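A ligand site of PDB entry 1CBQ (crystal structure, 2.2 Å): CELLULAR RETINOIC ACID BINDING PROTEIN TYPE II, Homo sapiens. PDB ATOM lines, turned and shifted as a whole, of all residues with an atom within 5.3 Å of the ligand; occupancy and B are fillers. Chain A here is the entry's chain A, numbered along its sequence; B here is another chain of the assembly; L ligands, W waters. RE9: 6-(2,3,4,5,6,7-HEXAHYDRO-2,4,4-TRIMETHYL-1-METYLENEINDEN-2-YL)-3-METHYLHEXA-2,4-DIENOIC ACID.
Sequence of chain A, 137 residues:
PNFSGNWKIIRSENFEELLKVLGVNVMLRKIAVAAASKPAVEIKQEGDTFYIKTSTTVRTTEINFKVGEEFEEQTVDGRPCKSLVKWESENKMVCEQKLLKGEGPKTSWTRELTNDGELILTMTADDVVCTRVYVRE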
ATOM      1  N   ILE A   9      -3.898   5.502 -15.769  1.00  0.00           N
ATOM      2  CA  ILE A   9      -4.237   4.105 -15.827  1.00  0.00           C
ATOM      3  C   ILE A   9      -5.676   3.810 -15.500  1.00  0.00           C
ATOM      4  O   ILE A   9      -6.303   4.511 -14.696  1.00  0.00           O
ATOM      5  CB  ILE A   9      -3.324   3.348 -14.912  1.00  0.00           C
ATOM      6  CG1 ILE A   9      -3.340   1.856 -15.255  1.00  0.00           C
ATOM      7  CG2 ILE A   9      -3.702   3.666 -13.470  1.00  0.00           C
ATOM      8  CD1 ILE A   9      -2.407   1.039 -14.424  1.00  0.00           C
ATOM      9  N   PHE A  15       0.926  -7.299 -12.110  1.00  0.00           N
ATOM     10  CA  PHE A  15       2.064  -6.456 -11.782  1.00  0.00           C
ATOM     11  C   PHE A  15       2.872  -7.007 -10.607  1.00  0.00           C
ATOM     12  O   PHE A  15       4.099  -7.028 -10.650  1.00  0.00           O
ATOM     13  CB  PHE A  15       1.616  -5.017 -11.491  1.00  0.00           C
ATOM     14  CG  PHE A  15       2.754  -4.081 -11.163  1.00  0.00           C
ATOM     15  CD1 PHE A  15       3.800  -3.885 -12.073  1.00  0.00           C
ATOM     16  CD2 PHE A  15       2.805  -3.428  -9.922  1.00  0.00           C
ATOM     17  CE1 PHE A  15       4.883  -3.063 -11.745  1.00  0.00           C
ATOM     18  CE2 PHE A  15       3.888  -2.606  -9.594  1.00  0.00           C
ATOM     19  CZ  PHE A  15       4.923  -2.418 -10.503  1.00  0.00           C
ATOM     20  N   LEU A  19       6.760  -8.800 -10.411  1.00  0.00           N
ATOM     21  CA  LEU A  19       7.771  -8.341  -9.467  1.00  0.00           C
ATOM     22  C   LEU A  19       8.304  -9.527  -8.665  1.00  0.00           C
ATOM     23  O   LEU A  19       9.486  -9.569  -8.338  1.00  0.00           O
ATOM     24  CB  LEU A  19       7.143  -7.328  -8.512  1.00  0.00           C
ATOM     25  CG  LEU A  19       7.299  -5.829  -8.773  1.00  0.00           C
ATOM     26  CD1 LEU A  19       7.688  -5.543 -10.202  1.00  0.00           C
ATOM     27  CD2 LEU A  19       6.022  -5.135  -8.362  1.00  0.00           C
ATOM     28  N   VAL A  24      11.770  -9.273  -6.461  1.00  0.00           N
ATOM     29  CA  VAL A  24      11.696  -8.048  -5.666  1.00  0.00           C
ATOM     30  C   VAL A  24      11.170  -8.492  -4.311  1.00  0.00           C
ATOM     31  O   VAL A  24      10.269  -9.338  -4.248  1.00  0.00           O
ATOM     32  CB  VAL A  24      10.760  -7.017  -6.316  1.00  0.00           C
ATOM     33  CG1 VAL A  24      10.633  -5.795  -5.453  1.00  0.00           C
ATOM     34  CG2 VAL A  24      11.326  -6.597  -7.634  1.00  0.00           C
ATOM     35  N   LEU A  28       9.562  -4.037  -0.782  1.00  0.00           N
ATOM     36  CA  LEU A  28       9.665  -3.246  -1.997  1.00  0.00           C
ATOM     37  C   LEU A  28       8.460  -3.459  -2.912  1.00  0.00           C
ATOM     38  O   LEU A  28       8.013  -2.532  -3.577  1.00  0.00           O
ATOM     39  CB  LEU A  28      10.973  -3.531  -2.735  1.00  0.00           C
ATOM     40  CG  LEU A  28      12.305  -3.167  -2.076  1.00  0.00           C
ATOM     41  CD1 LEU A  28      13.376  -3.311  -3.118  1.00  0.00           C
ATOM     42  CD2 LEU A  28      12.295  -1.752  -1.520  1.00  0.00           C
ATOM     43  N   ILE A  31       5.529  -1.386  -1.660  1.00  0.00           N
ATOM     44  CA  ILE A  31       5.692   0.017  -1.966  1.00  0.00           C
ATOM     45  C   ILE A  31       5.438   0.223  -3.467  1.00  0.00           C
ATOM     46  O   ILE A  31       4.788   1.185  -3.851  1.00  0.00           O
ATOM     47  CB  ILE A  31       7.129   0.489  -1.588  1.00  0.00           C
ATOM     48  CG1 ILE A  31       7.339   0.351  -0.081  1.00  0.00           C
ATOM     49  CG2 ILE A  31       7.335   1.931  -1.973  1.00  0.00           C
ATOM     50  CD1 ILE A  31       8.705   0.843   0.365  1.00  0.00           C
ATOM     51  N   ALA A  32       5.929  -0.687  -4.293  1.00  0.00           N
ATOM     52  CA  ALA A  32       5.784  -0.592  -5.744  1.00  0.00           C
ATOM     53  C   ALA A  32       4.343  -0.655  -6.151  1.00  0.00           C
ATOM     54  O   ALA A  32       3.894   0.101  -6.994  1.00  0.00           O
ATOM     55  CB  ALA A  32       6.551  -1.703  -6.420  1.00  0.00           C
ATOM     56  N   ALA A  35       2.513   2.574  -5.146  1.00  0.00           N
ATOM     57  CA  ALA A  35       2.924   3.702  -5.973  1.00  0.00           C
ATOM     58  C   ALA A  35       2.461   3.583  -7.417  1.00  0.00           C
ATOM     59  O   ALA A  35       2.102   4.578  -8.026  1.00  0.00           O
ATOM     60  CB  ALA A  35       4.447   3.857  -5.909  1.00  0.00           C
ATOM     61  N   ALA A  36       2.462   2.367  -7.976  1.00  0.00           N
ATOM     62  CA  ALA A  36       2.045   2.136  -9.364  1.00  0.00           C
ATOM     63  C   ALA A  36       0.529   2.282  -9.550  1.00  0.00           C
ATOM     64  O   ALA A  36       0.005   2.248 -10.679  1.00  0.00           O
ATOM     65  CB  ALA A  36       2.497   0.756  -9.801  1.00  0.00           C
ATOM     66  N   PRO A  39      -0.016   6.291 -11.442  1.00  0.00           N
ATOM     67  CA  PRO A  39       1.150   6.933 -12.034  1.00  0.00           C
ATOM     68  C   PRO A  39       0.698   8.039 -12.985  1.00  0.00           C
ATOM     69  O   PRO A  39      -0.493   8.263 -13.170  1.00  0.00           O
ATOM     70  CB  PRO A  39       1.827   5.778 -12.780  1.00  0.00           C
ATOM     71  CG  PRO A  39       0.690   4.928 -13.238  1.00  0.00           C
ATOM     72  CD  PRO A  39      -0.341   5.019 -12.114  1.00  0.00           C
ATOM     73  N   VAL A  41       1.846   9.154 -16.755  1.00  0.00           N
ATOM     74  CA  VAL A  41       2.713   8.845 -17.885  1.00  0.00           C
ATOM     75  C   VAL A  41       2.667   9.974 -18.892  1.00  0.00           C
ATOM     76  O   VAL A  41       1.595  10.371 -19.336  1.00  0.00           O
ATOM     77  CB  VAL A  41       2.277   7.527 -18.590  1.00  0.00           C
ATOM     78  CG1 VAL A  41       3.203   7.209 -19.728  1.00  0.00           C
ATOM     79  CG2 VAL A  41       2.264   6.379 -17.592  1.00  0.00           C
ATOM     80  N   THR A  54       7.568   8.320 -16.613  1.00  0.00           N
ATOM     81  CA  THR A  54       6.594   7.621 -15.790  1.00  0.00           C
ATOM     82  C   THR A  54       6.818   8.041 -14.345  1.00  0.00           C
ATOM     83  O   THR A  54       7.800   7.624 -13.710  1.00  0.00           O
ATOM     84  CB  THR A  54       6.741   6.094 -15.932  1.00  0.00           C
ATOM     85  OG1 THR A  54       6.567   5.712 -17.297  1.00  0.00           O
ATOM     86  CG2 THR A  54       5.701   5.382 -15.082  1.00  0.00           C
ATOM     87  N   THR A  56       5.589   8.478 -10.297  1.00  0.00           N
ATOM     88  CA  THR A  56       4.831   7.934  -9.179  1.00  0.00           C
ATOM     89  C   THR A  56       5.375   8.818  -8.032  1.00  0.00           C
ATOM     90  O   THR A  56       6.316   9.592  -8.242  1.00  0.00           O
ATOM     91  CB  THR A  56       5.024   6.408  -8.938  1.00  0.00           C
ATOM     92  OG1 THR A  56       6.320   6.162  -8.404  1.00  0.00           O
ATOM     93  CG2 THR A  56       4.844   5.623 -10.238  1.00  0.00           C
ATOM     94  N   VAL A  58       6.914   7.967  -5.409  1.00  0.00           N
ATOM     95  CA  VAL A  58       8.132   7.412  -4.809  1.00  0.00           C
ATOM     96  C   VAL A  58       9.292   7.234  -5.757  1.00  0.00           C
ATOM     97  O   VAL A  58      10.435   7.392  -5.360  1.00  0.00           O
ATOM     98  CB  VAL A  58       7.850   6.031  -4.186  1.00  0.00           C
ATOM     99  CG1 VAL A  58       9.102   5.453  -3.602  1.00  0.00           C
ATOM    100  CG2 VAL A  58       6.795   6.142  -3.146  1.00  0.00           C
ATOM    101  N   ARG A  59       8.999   6.882  -7.006  1.00  0.00           N
ATOM    102  CA  ARG A  59      10.063   6.652  -7.971  1.00  0.00           C
ATOM    103  C   ARG A  59       9.597   6.987  -9.358  1.00  0.00           C
ATOM    104  O   ARG A  59       8.533   6.534  -9.795  1.00  0.00           O
ATOM    105  CB  ARG A  59      10.485   5.190  -7.897  1.00  0.00           C
ATOM    106  CG  ARG A  59      11.461   4.784  -8.943  1.00  0.00           C
ATOM    107  CD  ARG A  59      12.004   3.446  -8.596  1.00  0.00           C
ATOM    108  NE  ARG A  59      12.615   2.803  -9.745  1.00  0.00           N
ATOM    109  CZ  ARG A  59      13.903   2.880 -10.038  1.00  0.00           C
ATOM    110  NH1 ARG A  59      14.739   3.590  -9.273  1.00  0.00           N
ATOM    111  NH2 ARG A  59      14.369   2.227 -11.105  1.00  0.00           N
ATOM    112  N   VAL A  76      12.246  -3.110 -14.920  1.00  0.00           N
ATOM    113  CA  VAL A  76      11.240  -2.575 -13.984  1.00  0.00           C
ATOM    114  C   VAL A  76      11.774  -2.598 -12.562  1.00  0.00           C
ATOM    115  O   VAL A  76      11.433  -1.733 -11.746  1.00  0.00           O
ATOM    116  CB  VAL A  76       9.928  -3.387 -13.935  1.00  0.00           C
ATOM    117  CG1 VAL A  76       8.738  -2.444 -13.777  1.00  0.00           C
ATOM    118  CG2 VAL A  76       9.800  -4.306 -15.122  1.00  0.00           C
ATOM    119  N   ASP A  77      12.563  -3.622 -12.252  1.00  0.00           N
ATOM    120  CA  ASP A  77      13.109  -3.753 -10.924  1.00  0.00           C
ATOM    121  C   ASP A  77      14.373  -2.942 -10.650  1.00  0.00           C
ATOM    122  O   ASP A  77      14.974  -3.063  -9.591  1.00  0.00           O
ATOM    123  CB  ASP A  77      13.274  -5.238 -10.548  1.00  0.00           C
ATOM    124  CG  ASP A  77      14.201  -5.981 -11.458  1.00  0.00           C
ATOM    125  OD1 ASP A  77      14.123  -5.795 -12.693  1.00  0.00           O
ATOM    126  OD2 ASP A  77      15.014  -6.778 -10.952  1.00  0.00           O
ATOM    127  N   GLY A  78      14.776  -2.109 -11.599  1.00  0.00           N
ATOM    128  CA  GLY A  78      15.919  -1.261 -11.357  1.00  0.00           C
ATOM    129  C   GLY A  78      17.260  -1.733 -11.850  1.00  0.00           C
ATOM    130  O   GLY A  78      18.261  -1.129 -11.498  1.00  0.00           O
ATOM    131  N   ARG A 111       4.377  -1.436 -26.135  1.00  0.00           N
ATOM    132  CA  ARG A 111       3.427  -0.339 -25.976  1.00  0.00           C
ATOM    133  C   ARG A 111       2.637  -0.316 -27.271  1.00  0.00           C
ATOM    134  O   ARG A 111       3.193  -0.413 -28.359  1.00  0.00           O
ATOM    135  CB  ARG A 111       4.136   0.974 -25.712  1.00  0.00           C
ATOM    136  CG  ARG A 111       4.505   1.147 -24.250  1.00  0.00           C
ATOM    137  CD  ARG A 111       5.093   2.502 -23.985  1.00  0.00           C
ATOM    138  NE  ARG A 111       5.205   2.705 -22.549  1.00  0.00           N
ATOM    139  CZ  ARG A 111       6.299   2.491 -21.833  1.00  0.00           C
ATOM    140  NH1 ARG A 111       7.424   2.081 -22.399  1.00  0.00           N
ATOM    141  NH2 ARG A 111       6.256   2.622 -20.531  1.00  0.00           N
ATOM    142  N   LEU A 121       0.328  -1.247 -22.254  1.00  0.00           N
ATOM    143  CA  LEU A 121       1.705  -1.527 -21.890  1.00  0.00           C
ATOM    144  C   LEU A 121       1.746  -2.961 -21.392  1.00  0.00           C
ATOM    145  O   LEU A 121       0.949  -3.352 -20.556  1.00  0.00           O
ATOM    146  CB  LEU A 121       2.151  -0.595 -20.737  1.00  0.00           C
ATOM    147  CG  LEU A 121       3.424  -0.966 -19.960  1.00  0.00           C
ATOM    148  CD1 LEU A 121       4.638  -0.835 -20.848  1.00  0.00           C
ATOM    149  CD2 LEU A 121       3.600  -0.133 -18.690  1.00  0.00           C
ATOM    150  N   MET A 123       4.435  -5.915 -19.908  1.00  0.00           N
ATOM    151  CA  MET A 123       5.794  -6.084 -19.405  1.00  0.00           C
ATOM    152  C   MET A 123       5.919  -7.552 -19.132  1.00  0.00           C
ATOM    153  O   MET A 123       5.042  -8.146 -18.514  1.00  0.00           O
ATOM    154  CB  MET A 123       6.015  -5.284 -18.113  1.00  0.00           C
ATOM    155  CG  MET A 123       5.978  -3.799 -18.280  1.00  0.00           C
ATOM    156  SD  MET A 123       6.291  -2.893 -16.765  1.00  0.00           S
ATOM    157  CE  MET A 123       4.766  -3.137 -15.922  1.00  0.00           C
ATOM    158  N   ARG A 132      -1.137  -3.372 -18.583  1.00  0.00           N
ATOM    159  CA  ARG A 132      -1.632  -2.148 -17.990  1.00  0.00           C
ATOM    160  C   ARG A 132      -2.256  -1.302 -19.093  1.00  0.00           C
ATOM    161  O   ARG A 132      -1.643  -1.058 -20.125  1.00  0.00           O
ATOM    162  CB  ARG A 132      -0.473  -1.434 -17.272  1.00  0.00           C
ATOM    163  CG  ARG A 132       0.022  -2.204 -16.072  1.00  0.00           C
ATOM    164  CD  ARG A 132       1.318  -1.678 -15.523  1.00  0.00           C
ATOM    165  NE  ARG A 132       1.199  -0.352 -14.947  1.00  0.00           N
ATOM    166  CZ  ARG A 132       0.723  -0.097 -13.727  1.00  0.00           C
ATOM    167  NH1 ARG A 132       0.303  -1.081 -12.948  1.00  0.00           N
ATOM    168  NH2 ARG A 132       0.759   1.140 -13.260  1.00  0.00           N
ATOM    169  N   TYR A 134      -4.148   2.315 -20.292  1.00  0.00           N
ATOM    170  CA  TYR A 134      -4.270   3.747 -19.999  1.00  0.00           C
ATOM    171  C   TYR A 134      -5.172   4.468 -21.000  1.00  0.00           C
ATOM    172  O   TYR A 134      -5.412   3.975 -22.096  1.00  0.00           O
ATOM    173  CB  TYR A 134      -2.895   4.424 -20.098  1.00  0.00           C
ATOM    174  CG  TYR A 134      -1.785   3.764 -19.334  1.00  0.00           C
ATOM    175  CD1 TYR A 134      -1.138   2.643 -19.850  1.00  0.00           C
ATOM    176  CD2 TYR A 134      -1.355   4.271 -18.107  1.00  0.00           C
ATOM    177  CE1 TYR A 134      -0.085   2.037 -19.152  1.00  0.00           C
ATOM    178  CE2 TYR A 134      -0.309   3.663 -17.397  1.00  0.00           C
ATOM    179  CZ  TYR A 134       0.319   2.541 -17.940  1.00  0.00           C
ATOM    180  OH  TYR A 134       1.304   1.895 -17.244  1.00  0.00           O
ATOM    181  N   THR B  57      16.781   0.919  -5.201  1.00  0.00           N
ATOM    182  CA  THR B  57      15.561   1.250  -5.928  1.00  0.00           C
ATOM    183  C   THR B  57      14.760   2.395  -5.341  1.00  0.00           C
ATOM    184  O   THR B  57      13.889   2.965  -6.014  1.00  0.00           O
ATOM    185  CB  THR B  57      14.669   0.018  -6.067  1.00  0.00           C
ATOM    186  OG1 THR B  57      14.581  -0.661  -4.807  1.00  0.00           O
ATOM    187  CG2 THR B  57      15.235  -0.937  -7.107  1.00  0.00           C
ATOM    188  N   VAL B  58      15.082   2.786  -4.112  1.00  0.00           N
ATOM    189  CA  VAL B  58      14.359   3.855  -3.416  1.00  0.00           C
ATOM    190  C   VAL B  58      15.149   5.117  -3.177  1.00  0.00           C
ATOM    191  O   VAL B  58      14.591   6.202  -3.207  1.00  0.00           O
ATOM    192  CB  VAL B  58      13.867   3.369  -2.038  1.00  0.00           C
ATOM    193  CG1 VAL B  58      13.156   4.472  -1.316  1.00  0.00           C
ATOM    194  CG2 VAL B  58      12.975   2.192  -2.196  1.00  0.00           C
HETATM  195  C1  RE9 L   1      10.563  -1.046  -7.655  1.00  0.00           C
HETATM  196  C2  RE9 L   1      10.725  -1.184  -6.102  1.00  0.00           C
HETATM  197  C3  RE9 L   1      10.888   0.207  -5.420  1.00  0.00           C
HETATM  198  C4  RE9 L   1       9.661   1.108  -5.603  1.00  0.00           C
HETATM  199  C5  RE9 L   1       9.149   1.006  -7.039  1.00  0.00           C
HETATM  200  C6  RE9 L   1       8.178   1.917  -7.623  1.00  0.00           C
HETATM  201  C7  RE9 L   1       7.928   1.517  -9.088  1.00  0.00           C
HETATM  202  C8  RE9 L   1       8.806   0.242  -9.280  1.00  0.00           C
HETATM  203  C9  RE9 L   1       9.532   0.060  -7.961  1.00  0.00           C
HETATM  204  C10 RE9 L   1       6.410   1.221  -9.284  1.00  0.00           C
HETATM  205  C11 RE9 L   1       6.188   0.971 -10.753  1.00  0.00           C
HETATM  206  C12 RE9 L   1       5.336   1.728 -11.503  1.00  0.00           C
HETATM  207  C13 RE9 L   1       4.979   1.522 -12.913  1.00  0.00           C
HETATM  208  C14 RE9 L   1       4.115   2.393 -13.441  1.00  0.00           C
HETATM  209  C15 RE9 L   1       3.574   2.423 -14.784  1.00  0.00           C
HETATM  210  C16 RE9 L   1      10.101  -2.373  -8.237  1.00  0.00           C
HETATM  211  C17 RE9 L   1      11.898  -0.719  -8.328  1.00  0.00           C
HETATM  212  C18 RE9 L   1       7.579   2.944  -6.983  1.00  0.00           C
HETATM  213  C19 RE9 L   1       8.376   2.508 -10.151  1.00  0.00           C
HETATM  214  C20 RE9 L   1       5.555   0.383 -13.648  1.00  0.00           C
HETATM  215  O1  RE9 L   1       4.311   2.233 -15.764  1.00  0.00           O
HETATM  216  O2  RE9 L   1       2.355   2.654 -14.927  1.00  0.00           O
HETATM  217  O   HOH W   1       4.492   3.650 -18.387  1.00  0.00           O
HETATM  218  O   HOH W   2       7.049   1.901 -16.491  1.00  0.00           O
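The guanidinium group (NH2) of Arg 132 lies within salt-bridge range of an oxygen (O2) of the ligand (2.8 Å). OH of Tyr 134 is in hydrogen-bond range of O2 of the ligand, at 2.7 Å.
The backbone carbonyl oxygen (O) of Leu 121 lies within hydrogen-bond range of the backbone NH (N) of Arg 132, at 2.9 Å. The backbone carbonyl oxygen (O) of Arg 59 is in hydrogen-bond range of the side-chain hydroxyl (OG1) of Thr 56, at 2.6 Å. NH2 of Arg 132 is in hydrogen-bond range of O of Ala 36 (2.9 Å). The side-chain hydroxyl of Tyr 134 is in hydrogen-bond range of the guanidinium group of Arg 132. O of Thr 57 of chain B sits close to NH1 of Arg 59 (3.4 Å).
Merely in contact with the ligand: Phe 15, Leu 28, Ala 32, Ala 35, Ala 36, Pro 39, Thr 54, Thr 56, Arg 59, Val 76, Leu 121 and Thr 57 of chain B. Hydrophobic or aromatic side chains that line the ligand: Phe 15, Ala 32, Ala 35, Ala 36, Pro 39, Leu 121 and Tyr 134.
Water W1 lies within hydrogen-bond range of NH2 of Arg 111, O1 of the ligand and OG1 of Thr 54.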
